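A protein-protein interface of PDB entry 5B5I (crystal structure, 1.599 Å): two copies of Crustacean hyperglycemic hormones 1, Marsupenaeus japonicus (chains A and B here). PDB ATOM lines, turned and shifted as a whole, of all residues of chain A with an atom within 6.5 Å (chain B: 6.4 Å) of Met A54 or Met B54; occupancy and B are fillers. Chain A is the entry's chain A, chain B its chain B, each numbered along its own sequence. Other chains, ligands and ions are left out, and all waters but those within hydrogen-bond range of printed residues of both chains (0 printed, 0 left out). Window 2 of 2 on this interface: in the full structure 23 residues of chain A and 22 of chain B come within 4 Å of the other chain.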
ATOM      1  N   LEU A  20      28.395  -5.266 -11.800  1.00  0.00           N
ATOM      2  CA  LEU A  20      28.200  -4.399 -12.948  1.00  0.00           C
ATOM      3  C   LEU A  20      29.162  -4.759 -14.068  1.00  0.00           C
ATOM      4  O   LEU A  20      28.799  -4.710 -15.248  1.00  0.00           O
ATOM      5  CB  LEU A  20      28.373  -2.940 -12.536  1.00  0.00           C
ATOM      6  CG  LEU A  20      27.385  -2.471 -11.481  1.00  0.00           C
ATOM      7  CD1 LEU A  20      27.899  -1.166 -10.901  1.00  0.00           C
ATOM      8  CD2 LEU A  20      25.990  -2.312 -12.048  1.00  0.00           C
ATOM      9  N   VAL A  23      27.914  -7.155 -16.695  1.00  0.00           N
ATOM     10  CA  VAL A  23      27.170  -6.648 -17.845  1.00  0.00           C
ATOM     11  C   VAL A  23      28.104  -6.476 -19.034  1.00  0.00           C
ATOM     12  O   VAL A  23      27.786  -6.873 -20.161  1.00  0.00           O
ATOM     13  CB  VAL A  23      26.452  -5.330 -17.495  1.00  0.00           C
ATOM     14  CG1 VAL A  23      25.842  -4.721 -18.741  1.00  0.00           C
ATOM     15  CG2 VAL A  23      25.371  -5.593 -16.458  1.00  0.00           C
ATOM     16  N   CYS A  27      28.359  -8.780 -22.630  1.00  0.00           N
ATOM     17  CA  CYS A  27      27.901  -8.024 -23.785  1.00  0.00           C
ATOM     18  C   CYS A  27      28.591  -8.453 -25.074  1.00  0.00           C
ATOM     19  O   CYS A  27      28.014  -8.321 -26.160  1.00  0.00           O
ATOM     20  CB  CYS A  27      28.126  -6.534 -23.529  1.00  0.00           C
ATOM     21  SG  CYS A  27      27.355  -5.451 -24.735  1.00  0.00           S
ATOM     22  N   VAL A  49      28.498   2.951 -23.659  1.00  0.00           N
ATOM     23  CA  VAL A  49      28.703   1.534 -23.973  1.00  0.00           C
ATOM     24  C   VAL A  49      28.003   0.666 -22.938  1.00  0.00           C
ATOM     25  O   VAL A  49      27.308  -0.300 -23.280  1.00  0.00           O
ATOM     26  CB  VAL A  49      30.204   1.201 -24.070  1.00  0.00           C
ATOM     27  CG1 VAL A  49      30.404  -0.300 -24.182  1.00  0.00           C
ATOM     28  CG2 VAL A  49      30.813   1.882 -25.278  1.00  0.00           C
ATOM     29  N   PHE A  50      28.168   0.996 -21.651  1.00  0.00           N
ATOM     30  CA  PHE A  50      27.475   0.238 -20.615  1.00  0.00           C
ATOM     31  C   PHE A  50      25.962   0.344 -20.780  1.00  0.00           C
ATOM     32  O   PHE A  50      25.241  -0.640 -20.606  1.00  0.00           O
ATOM     33  CB  PHE A  50      27.896   0.702 -19.217  1.00  0.00           C
ATOM     34  CG  PHE A  50      27.168  -0.003 -18.103  1.00  0.00           C
ATOM     35  CD1 PHE A  50      25.955   0.485 -17.631  1.00  0.00           C
ATOM     36  CD2 PHE A  50      27.686  -1.164 -17.532  1.00  0.00           C
ATOM     37  CE1 PHE A  50      25.278  -0.172 -16.602  1.00  0.00           C
ATOM     38  CE2 PHE A  50      27.012  -1.822 -16.505  1.00  0.00           C
ATOM     39  CZ  PHE A  50      25.802  -1.320 -16.041  1.00  0.00           C
ATOM     40  N   ARG A  51      25.455   1.537 -21.093  1.00  0.00           N
ATOM     41  CA  ARG A  51      24.008   1.649 -21.243  1.00  0.00           C
ATOM     42  C   ARG A  51      23.506   0.820 -22.419  1.00  0.00           C
ATOM     43  O   ARG A  51      22.450   0.184 -22.326  1.00  0.00           O
ATOM     44  CB  ARG A  51      23.597   3.112 -21.397  1.00  0.00           C
ATOM     45  CG  ARG A  51      23.702   3.894 -20.114  1.00  0.00           C
ATOM     46  CD  ARG A  51      23.177   5.319 -20.297  1.00  0.00           C
ATOM     47  NE  ARG A  51      24.028   6.128 -21.159  1.00  0.00           N
ATOM     48  CZ  ARG A  51      24.992   6.928 -20.718  1.00  0.00           C
ATOM     49  NH1 ARG A  51      25.243   7.012 -19.418  1.00  0.00           N
ATOM     50  NH2 ARG A  51      25.718   7.633 -21.581  1.00  0.00           N
ATOM     51  N   GLN A  52      24.241   0.810 -23.537  1.00  0.00           N
ATOM     52  CA  GLN A  52      23.799   0.001 -24.669  1.00  0.00           C
ATOM     53  C   GLN A  52      23.928  -1.483 -24.358  1.00  0.00           C
ATOM     54  O   GLN A  52      23.063  -2.284 -24.731  1.00  0.00           O
ATOM     55  CB  GLN A  52      24.595   0.347 -25.922  1.00  0.00           C
ATOM     56  CG  GLN A  52      24.050  -0.302 -27.199  1.00  0.00           C
ATOM     57  CD  GLN A  52      22.629   0.127 -27.514  1.00  0.00           C
ATOM     58  OE1 GLN A  52      22.317   1.320 -27.541  1.00  0.00           O
ATOM     59  NE2 GLN A  52      21.758  -0.843 -27.752  1.00  0.00           N
ATOM     60  N   CYS A  53      25.013  -1.872 -23.693  1.00  0.00           N
ATOM     61  CA  CYS A  53      25.162  -3.269 -23.298  1.00  0.00           C
ATOM     62  C   CYS A  53      24.036  -3.724 -22.379  1.00  0.00           C
ATOM     63  O   CYS A  53      23.504  -4.825 -22.547  1.00  0.00           O
ATOM     64  CB  CYS A  53      26.520  -3.474 -22.640  1.00  0.00           C
ATOM     65  SG  CYS A  53      27.798  -3.650 -23.912  1.00  0.00           S
ATOM     66  N   MET A  54      23.665  -2.894 -21.401  1.00  0.00           N
ATOM     67  CA  MET A  54      22.553  -3.222 -20.512  1.00  0.00           C
ATOM     68  C   MET A  54      21.259  -3.408 -21.307  1.00  0.00           C
ATOM     69  O   MET A  54      20.452  -4.294 -20.993  1.00  0.00           O
ATOM     70  CB  MET A  54      22.451  -2.126 -19.418  1.00  0.00           C
ATOM     71  CG  MET A  54      21.139  -2.001 -18.691  1.00  0.00           C
ATOM     72  SD  MET A  54      21.574  -1.508 -16.992  1.00  0.00           S
ATOM     73  CE  MET A  54      22.621  -3.013 -16.873  1.00  0.00           C
ATOM     74  N   ALA A  55      21.087  -2.645 -22.390  1.00  0.00           N
ATOM     75  CA  ALA A  55      19.912  -2.782 -23.246  1.00  0.00           C
ATOM     76  C   ALA A  55      19.866  -4.108 -23.995  1.00  0.00           C
ATOM     77  O   ALA A  55      18.779  -4.530 -24.415  1.00  0.00           O
ATOM     78  CB  ALA A  55      19.863  -1.620 -24.242  1.00  0.00           C
ATOM     79  N   TYR A  56      21.018  -4.759 -24.200  1.00  0.00           N
ATOM     80  CA  TYR A  56      21.066  -6.076 -24.821  1.00  0.00           C
ATOM     81  C   TYR A  56      21.058  -7.188 -23.779  1.00  0.00           C
ATOM     82  O   TYR A  56      20.322  -8.174 -23.913  1.00  0.00           O
ATOM     83  CB  TYR A  56      22.326  -6.231 -25.689  1.00  0.00           C
ATOM     84  CG  TYR A  56      22.453  -5.295 -26.869  1.00  0.00           C
ATOM     85  CD1 TYR A  56      21.398  -5.080 -27.735  1.00  0.00           C
ATOM     86  CD2 TYR A  56      23.670  -4.670 -27.153  1.00  0.00           C
ATOM     87  CE1 TYR A  56      21.539  -4.233 -28.834  1.00  0.00           C
ATOM     88  CE2 TYR A  56      23.817  -3.822 -28.240  1.00  0.00           C
ATOM     89  CZ  TYR A  56      22.747  -3.610 -29.082  1.00  0.00           C
ATOM     90  OH  TYR A  56      22.863  -2.772 -30.167  1.00  0.00           O
ATOM     91  N   VAL A  57      21.880  -7.032 -22.738  1.00  0.00           N
ATOM     92  CA  VAL A  57      22.134  -8.096 -21.779  1.00  0.00           C
ATOM     93  C   VAL A  57      20.943  -8.302 -20.851  1.00  0.00           C
ATOM     94  O   VAL A  57      20.553  -9.439 -20.565  1.00  0.00           O
ATOM     95  CB  VAL A  57      23.419  -7.772 -20.993  1.00  0.00           C
ATOM     96  CG1 VAL A  57      23.562  -8.709 -19.812  1.00  0.00           C
ATOM     97  CG2 VAL A  57      24.640  -7.834 -21.934  1.00  0.00           C
ATOM     98  N   VAL A  58      20.334  -7.220 -20.363  1.00  0.00           N
ATOM     99  CA  VAL A  58      19.199  -7.379 -19.447  1.00  0.00           C
ATOM    100  C   VAL A  58      18.022  -8.093 -20.112  1.00  0.00           C
ATOM    101  O   VAL A  58      17.527  -9.079 -19.542  1.00  0.00           O
ATOM    102  CB  VAL A  58      18.815  -6.028 -18.824  1.00  0.00           C
ATOM    103  CG1 VAL A  58      17.428  -6.117 -18.222  1.00  0.00           C
ATOM    104  CG2 VAL A  58      19.828  -5.645 -17.776  1.00  0.00           C
ATOM    105  N   PRO A  59      17.539  -7.677 -21.292  1.00  0.00           N
ATOM    106  CA  PRO A  59      16.430  -8.433 -21.906  1.00  0.00           C
ATOM    107  C   PRO A  59      16.798  -9.867 -22.251  1.00  0.00           C
ATOM    108  O   PRO A  59      15.957 -10.766 -22.108  1.00  0.00           O
ATOM    109  CB  PRO A  59      16.092  -7.611 -23.158  1.00  0.00           C
ATOM    110  CG  PRO A  59      16.610  -6.247 -22.866  1.00  0.00           C
ATOM    111  CD  PRO A  59      17.840  -6.447 -22.049  1.00  0.00           C
ATOM    112  N   LEU B  20      15.843  -5.388 -10.735  1.00  0.00           N
ATOM    113  CA  LEU B  20      15.778  -4.126 -11.460  1.00  0.00           C
ATOM    114  C   LEU B  20      14.728  -3.201 -10.861  1.00  0.00           C
ATOM    115  O   LEU B  20      14.917  -1.983 -10.809  1.00  0.00           O
ATOM    116  CB  LEU B  20      15.481  -4.388 -12.935  1.00  0.00           C
ATOM    117  CG  LEU B  20      16.538  -5.196 -13.672  1.00  0.00           C
ATOM    118  CD1 LEU B  20      15.911  -5.773 -14.937  1.00  0.00           C
ATOM    119  CD2 LEU B  20      17.718  -4.298 -13.993  1.00  0.00           C
ATOM    120  N   VAL B  23      15.984  -0.800  -8.239  1.00  0.00           N
ATOM    121  CA  VAL B  23      16.591   0.456  -8.692  1.00  0.00           C
ATOM    122  C   VAL B  23      15.570   1.587  -8.642  1.00  0.00           C
ATOM    123  O   VAL B  23      15.834   2.679  -8.115  1.00  0.00           O
ATOM    124  CB  VAL B  23      17.162   0.293 -10.111  1.00  0.00           C
ATOM    125  CG1 VAL B  23      17.664   1.642 -10.659  1.00  0.00           C
ATOM    126  CG2 VAL B  23      18.269  -0.747 -10.126  1.00  0.00           C
ATOM    127  N   CYS B  27      15.212   4.896  -5.861  1.00  0.00           N
ATOM    128  CA  CYS B  27      15.496   6.162  -6.514  1.00  0.00           C
ATOM    129  C   CYS B  27      14.701   7.321  -5.935  1.00  0.00           C
ATOM    130  O   CYS B  27      15.145   8.466  -6.022  1.00  0.00           O
ATOM    131  CB  CYS B  27      15.204   6.011  -8.004  1.00  0.00           C
ATOM    132  SG  CYS B  27      15.631   7.443  -9.015  1.00  0.00           S
ATOM    133  N   VAL B  49      13.697   7.152 -17.326  1.00  0.00           N
ATOM    134  CA  VAL B  49      13.592   7.267 -15.871  1.00  0.00           C
ATOM    135  C   VAL B  49      14.463   6.211 -15.196  1.00  0.00           C
ATOM    136  O   VAL B  49      15.218   6.506 -14.256  1.00  0.00           O
ATOM    137  CB  VAL B  49      12.122   7.158 -15.429  1.00  0.00           C
ATOM    138  CG1 VAL B  49      12.046   7.038 -13.924  1.00  0.00           C
ATOM    139  CG2 VAL B  49      11.328   8.389 -15.906  1.00  0.00           C
ATOM    140  N   PHE B  50      14.379   4.963 -15.666  1.00  0.00           N
ATOM    141  CA  PHE B  50      15.266   3.932 -15.127  1.00  0.00           C
ATOM    142  C   PHE B  50      16.733   4.300 -15.332  1.00  0.00           C
ATOM    143  O   PHE B  50      17.559   4.132 -14.425  1.00  0.00           O
ATOM    144  CB  PHE B  50      14.969   2.575 -15.764  1.00  0.00           C
ATOM    145  CG  PHE B  50      15.839   1.473 -15.243  1.00  0.00           C
ATOM    146  CD1 PHE B  50      15.502   0.798 -14.075  1.00  0.00           C
ATOM    147  CD2 PHE B  50      17.008   1.122 -15.906  1.00  0.00           C
ATOM    148  CE1 PHE B  50      16.312  -0.204 -13.590  1.00  0.00           C
ATOM    149  CE2 PHE B  50      17.815   0.106 -15.421  1.00  0.00           C
ATOM    150  CZ  PHE B  50      17.470  -0.551 -14.264  1.00  0.00           C
ATOM    151  N   ARG B  51      17.083   4.794 -16.524  1.00  0.00           N
ATOM    152  CA  ARG B  51      18.487   5.095 -16.793  1.00  0.00           C
ATOM    153  C   ARG B  51      19.009   6.210 -15.897  1.00  0.00           C
ATOM    154  O   ARG B  51      20.137   6.139 -15.392  1.00  0.00           O
ATOM    155  CB  ARG B  51      18.669   5.468 -18.260  1.00  0.00           C
ATOM    156  CG  ARG B  51      18.724   4.282 -19.180  1.00  0.00           C
ATOM    157  CD  ARG B  51      19.168   4.708 -20.573  1.00  0.00           C
ATOM    158  NE  ARG B  51      18.121   5.408 -21.308  1.00  0.00           N
ATOM    159  CZ  ARG B  51      17.155   4.797 -21.986  1.00  0.00           C
ATOM    160  NH1 ARG B  51      17.098   3.474 -22.008  1.00  0.00           N
ATOM    161  NH2 ARG B  51      16.240   5.505 -22.632  1.00  0.00           N
ATOM    162  N   GLN B  52      18.209   7.260 -15.704  1.00  0.00           N
ATOM    163  CA  GLN B  52      18.637   8.335 -14.814  1.00  0.00           C
ATOM    164  C   GLN B  52      18.664   7.858 -13.365  1.00  0.00           C
ATOM    165  O   GLN B  52      19.568   8.223 -12.607  1.00  0.00           O
ATOM    166  CB  GLN B  52      17.720   9.546 -14.964  1.00  0.00           C
ATOM    167  CG  GLN B  52      18.111  10.727 -14.078  1.00  0.00           C
ATOM    168  CD  GLN B  52      19.489  11.258 -14.405  1.00  0.00           C
ATOM    169  OE1 GLN B  52      19.720  11.770 -15.502  1.00  0.00           O
ATOM    170  NE2 GLN B  52      20.420  11.111 -13.472  1.00  0.00           N
ATOM    171  N   CYS B  53      17.675   7.045 -12.966  1.00  0.00           N
ATOM    172  CA  CYS B  53      17.701   6.452 -11.630  1.00  0.00           C
ATOM    173  C   CYS B  53      18.944   5.587 -11.429  1.00  0.00           C
ATOM    174  O   CYS B  53      19.574   5.649 -10.362  1.00  0.00           O
ATOM    175  CB  CYS B  53      16.414   5.662 -11.377  1.00  0.00           C
ATOM    176  SG  CYS B  53      15.049   6.754 -10.865  1.00  0.00           S
ATOM    177  N   MET B  54      19.302   4.765 -12.434  1.00  0.00           N
ATOM    178  CA  MET B  54      20.579   4.048 -12.461  1.00  0.00           C
ATOM    179  C   MET B  54      21.703   4.963 -12.030  1.00  0.00           C
ATOM    180  O   MET B  54      22.533   4.604 -11.186  1.00  0.00           O
ATOM    181  CB  MET B  54      20.909   3.539 -13.877  1.00  0.00           C
ATOM    182  CG  MET B  54      20.305   2.191 -14.354  1.00  0.00           C
ATOM    183  SD  MET B  54      21.460   0.744 -14.428  1.00  0.00           S
ATOM    184  CE  MET B  54      20.934   0.342 -12.731  1.00  0.00           C
ATOM    185  N   ALA B  55      21.752   6.139 -12.658  1.00  0.00           N
ATOM    186  CA  ALA B  55      22.893   7.029 -12.529  1.00  0.00           C
ATOM    187  C   ALA B  55      22.980   7.645 -11.144  1.00  0.00           C
ATOM    188  O   ALA B  55      24.070   8.053 -10.739  1.00  0.00           O
ATOM    189  CB  ALA B  55      22.833   8.114 -13.610  1.00  0.00           C
ATOM    190  N   TYR B  56      21.869   7.697 -10.404  1.00  0.00           N
ATOM    191  CA  TYR B  56      21.868   8.119  -9.009  1.00  0.00           C
ATOM    192  C   TYR B  56      22.096   6.948  -8.060  1.00  0.00           C
ATOM    193  O   TYR B  56      22.900   7.050  -7.129  1.00  0.00           O
ATOM    194  CB  TYR B  56      20.536   8.782  -8.644  1.00  0.00           C
ATOM    195  CG  TYR B  56      20.222  10.043  -9.388  1.00  0.00           C
ATOM    196  CD1 TYR B  56      21.174  11.041  -9.551  1.00  0.00           C
ATOM    197  CD2 TYR B  56      18.954  10.246  -9.916  1.00  0.00           C
ATOM    198  CE1 TYR B  56      20.863  12.217 -10.236  1.00  0.00           C
ATOM    199  CE2 TYR B  56      18.637  11.413 -10.601  1.00  0.00           C
ATOM    200  CZ  TYR B  56      19.589  12.388 -10.747  1.00  0.00           C
ATOM    201  OH  TYR B  56      19.281  13.554 -11.407  1.00  0.00           O
ATOM    202  N   VAL B  57      21.392   5.835  -8.297  1.00  0.00           N
ATOM    203  CA  VAL B  57      21.330   4.727  -7.346  1.00  0.00           C
ATOM    204  C   VAL B  57      22.620   3.926  -7.338  1.00  0.00           C
ATOM    205  O   VAL B  57      23.104   3.535  -6.272  1.00  0.00           O
ATOM    206  CB  VAL B  57      20.118   3.834  -7.664  1.00  0.00           C
ATOM    207  CG1 VAL B  57      20.178   2.528  -6.867  1.00  0.00           C
ATOM    208  CG2 VAL B  57      18.836   4.570  -7.313  1.00  0.00           C
ATOM    209  N   VAL B  58      23.184   3.640  -8.515  1.00  0.00           N
ATOM    210  CA  VAL B  58      24.398   2.828  -8.563  1.00  0.00           C
ATOM    211  C   VAL B  58      25.565   3.533  -7.886  1.00  0.00           C
ATOM    212  O   VAL B  58      26.210   2.915  -7.026  1.00  0.00           O
ATOM    213  CB  VAL B  58      24.715   2.411 -10.006  1.00  0.00           C
ATOM    214  CG1 VAL B  58      26.131   1.891 -10.064  1.00  0.00           C
ATOM    215  CG2 VAL B  58      23.750   1.355 -10.462  1.00  0.00           C
ATOM    216  N   PRO B  59      25.896   4.793  -8.218  1.00  0.00           N
ATOM    217  CA  PRO B  59      26.963   5.479  -7.475  1.00  0.00           C
ATOM    218  C   PRO B  59      26.703   5.534  -5.991  1.00  0.00           C
ATOM    219  O   PRO B  59      27.636   5.306  -5.212  1.00  0.00           O
ATOM    220  CB  PRO B  59      26.982   6.877  -8.104  1.00  0.00           C
ATOM    221  CG  PRO B  59      26.544   6.642  -9.478  1.00  0.00           C
ATOM    222  CD  PRO B  59      25.465   5.603  -9.376  1.00  0.00           C
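Leu A20 touches Val B58, and with the chains exchanged Val A58 touches Leu B20. Met A54 touches its own counterpart, Met B54. Of the 3 pairs that touch across the chains among the printed residues, 3 have their exchanged pair printed and touching as well.
Hydrophobic or aromatic side chains of chain A that line the printed part of chain B: Leu A20, Met A54 and Val A58. Of the 14 printed residues of chain B, 3 touch a printed residue of chain A. Printed residues of chain B that touch a printed residue of chain A: Leu B20, Met B54 and Val B58. Hydrophobic or aromatic side chains of chain B within 4 Å of the printed part of chain A: Leu B20, Met B54 and Val B58. Along chain B the printed residues that touch a printed residue of chain A span positions 20 to 58. Among the printed residues, 3 pairs touch across the chains. Among the printed residues, no Asp or Glu carboxylate lies within 4 Å of a Lys or Arg side-chain nitrogen of the other chain.
The side-chain sulfur of Cys A27 is disulfide-bonded to the side-chain sulfur of Cys A53. SG of Cys B53 is disulfide-bonded to SG of Cys B27, at 2.1 Å.
Among the printed residues, pairs that only touch across the chains: Leu A20 with Val B58 (3.6 Å) and Val A58 with Leu B20 (3.6 Å).
Of chain B, only Met B54 comes within 4 Å of Met A54. Of the printed residues of chain A, Val B58 touches Leu A20 (3.6 Å). Of the printed residues of chain A, Leu B20 touches Val A58 (3.6 Å). Printed residues of chain B within 4 Å of Val A58: Leu B20. Cys A27 touches none of the printed residues of chain B.
The side-chain sulfur of Met B54 lies close to the side-chain sulfur of Met A54.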
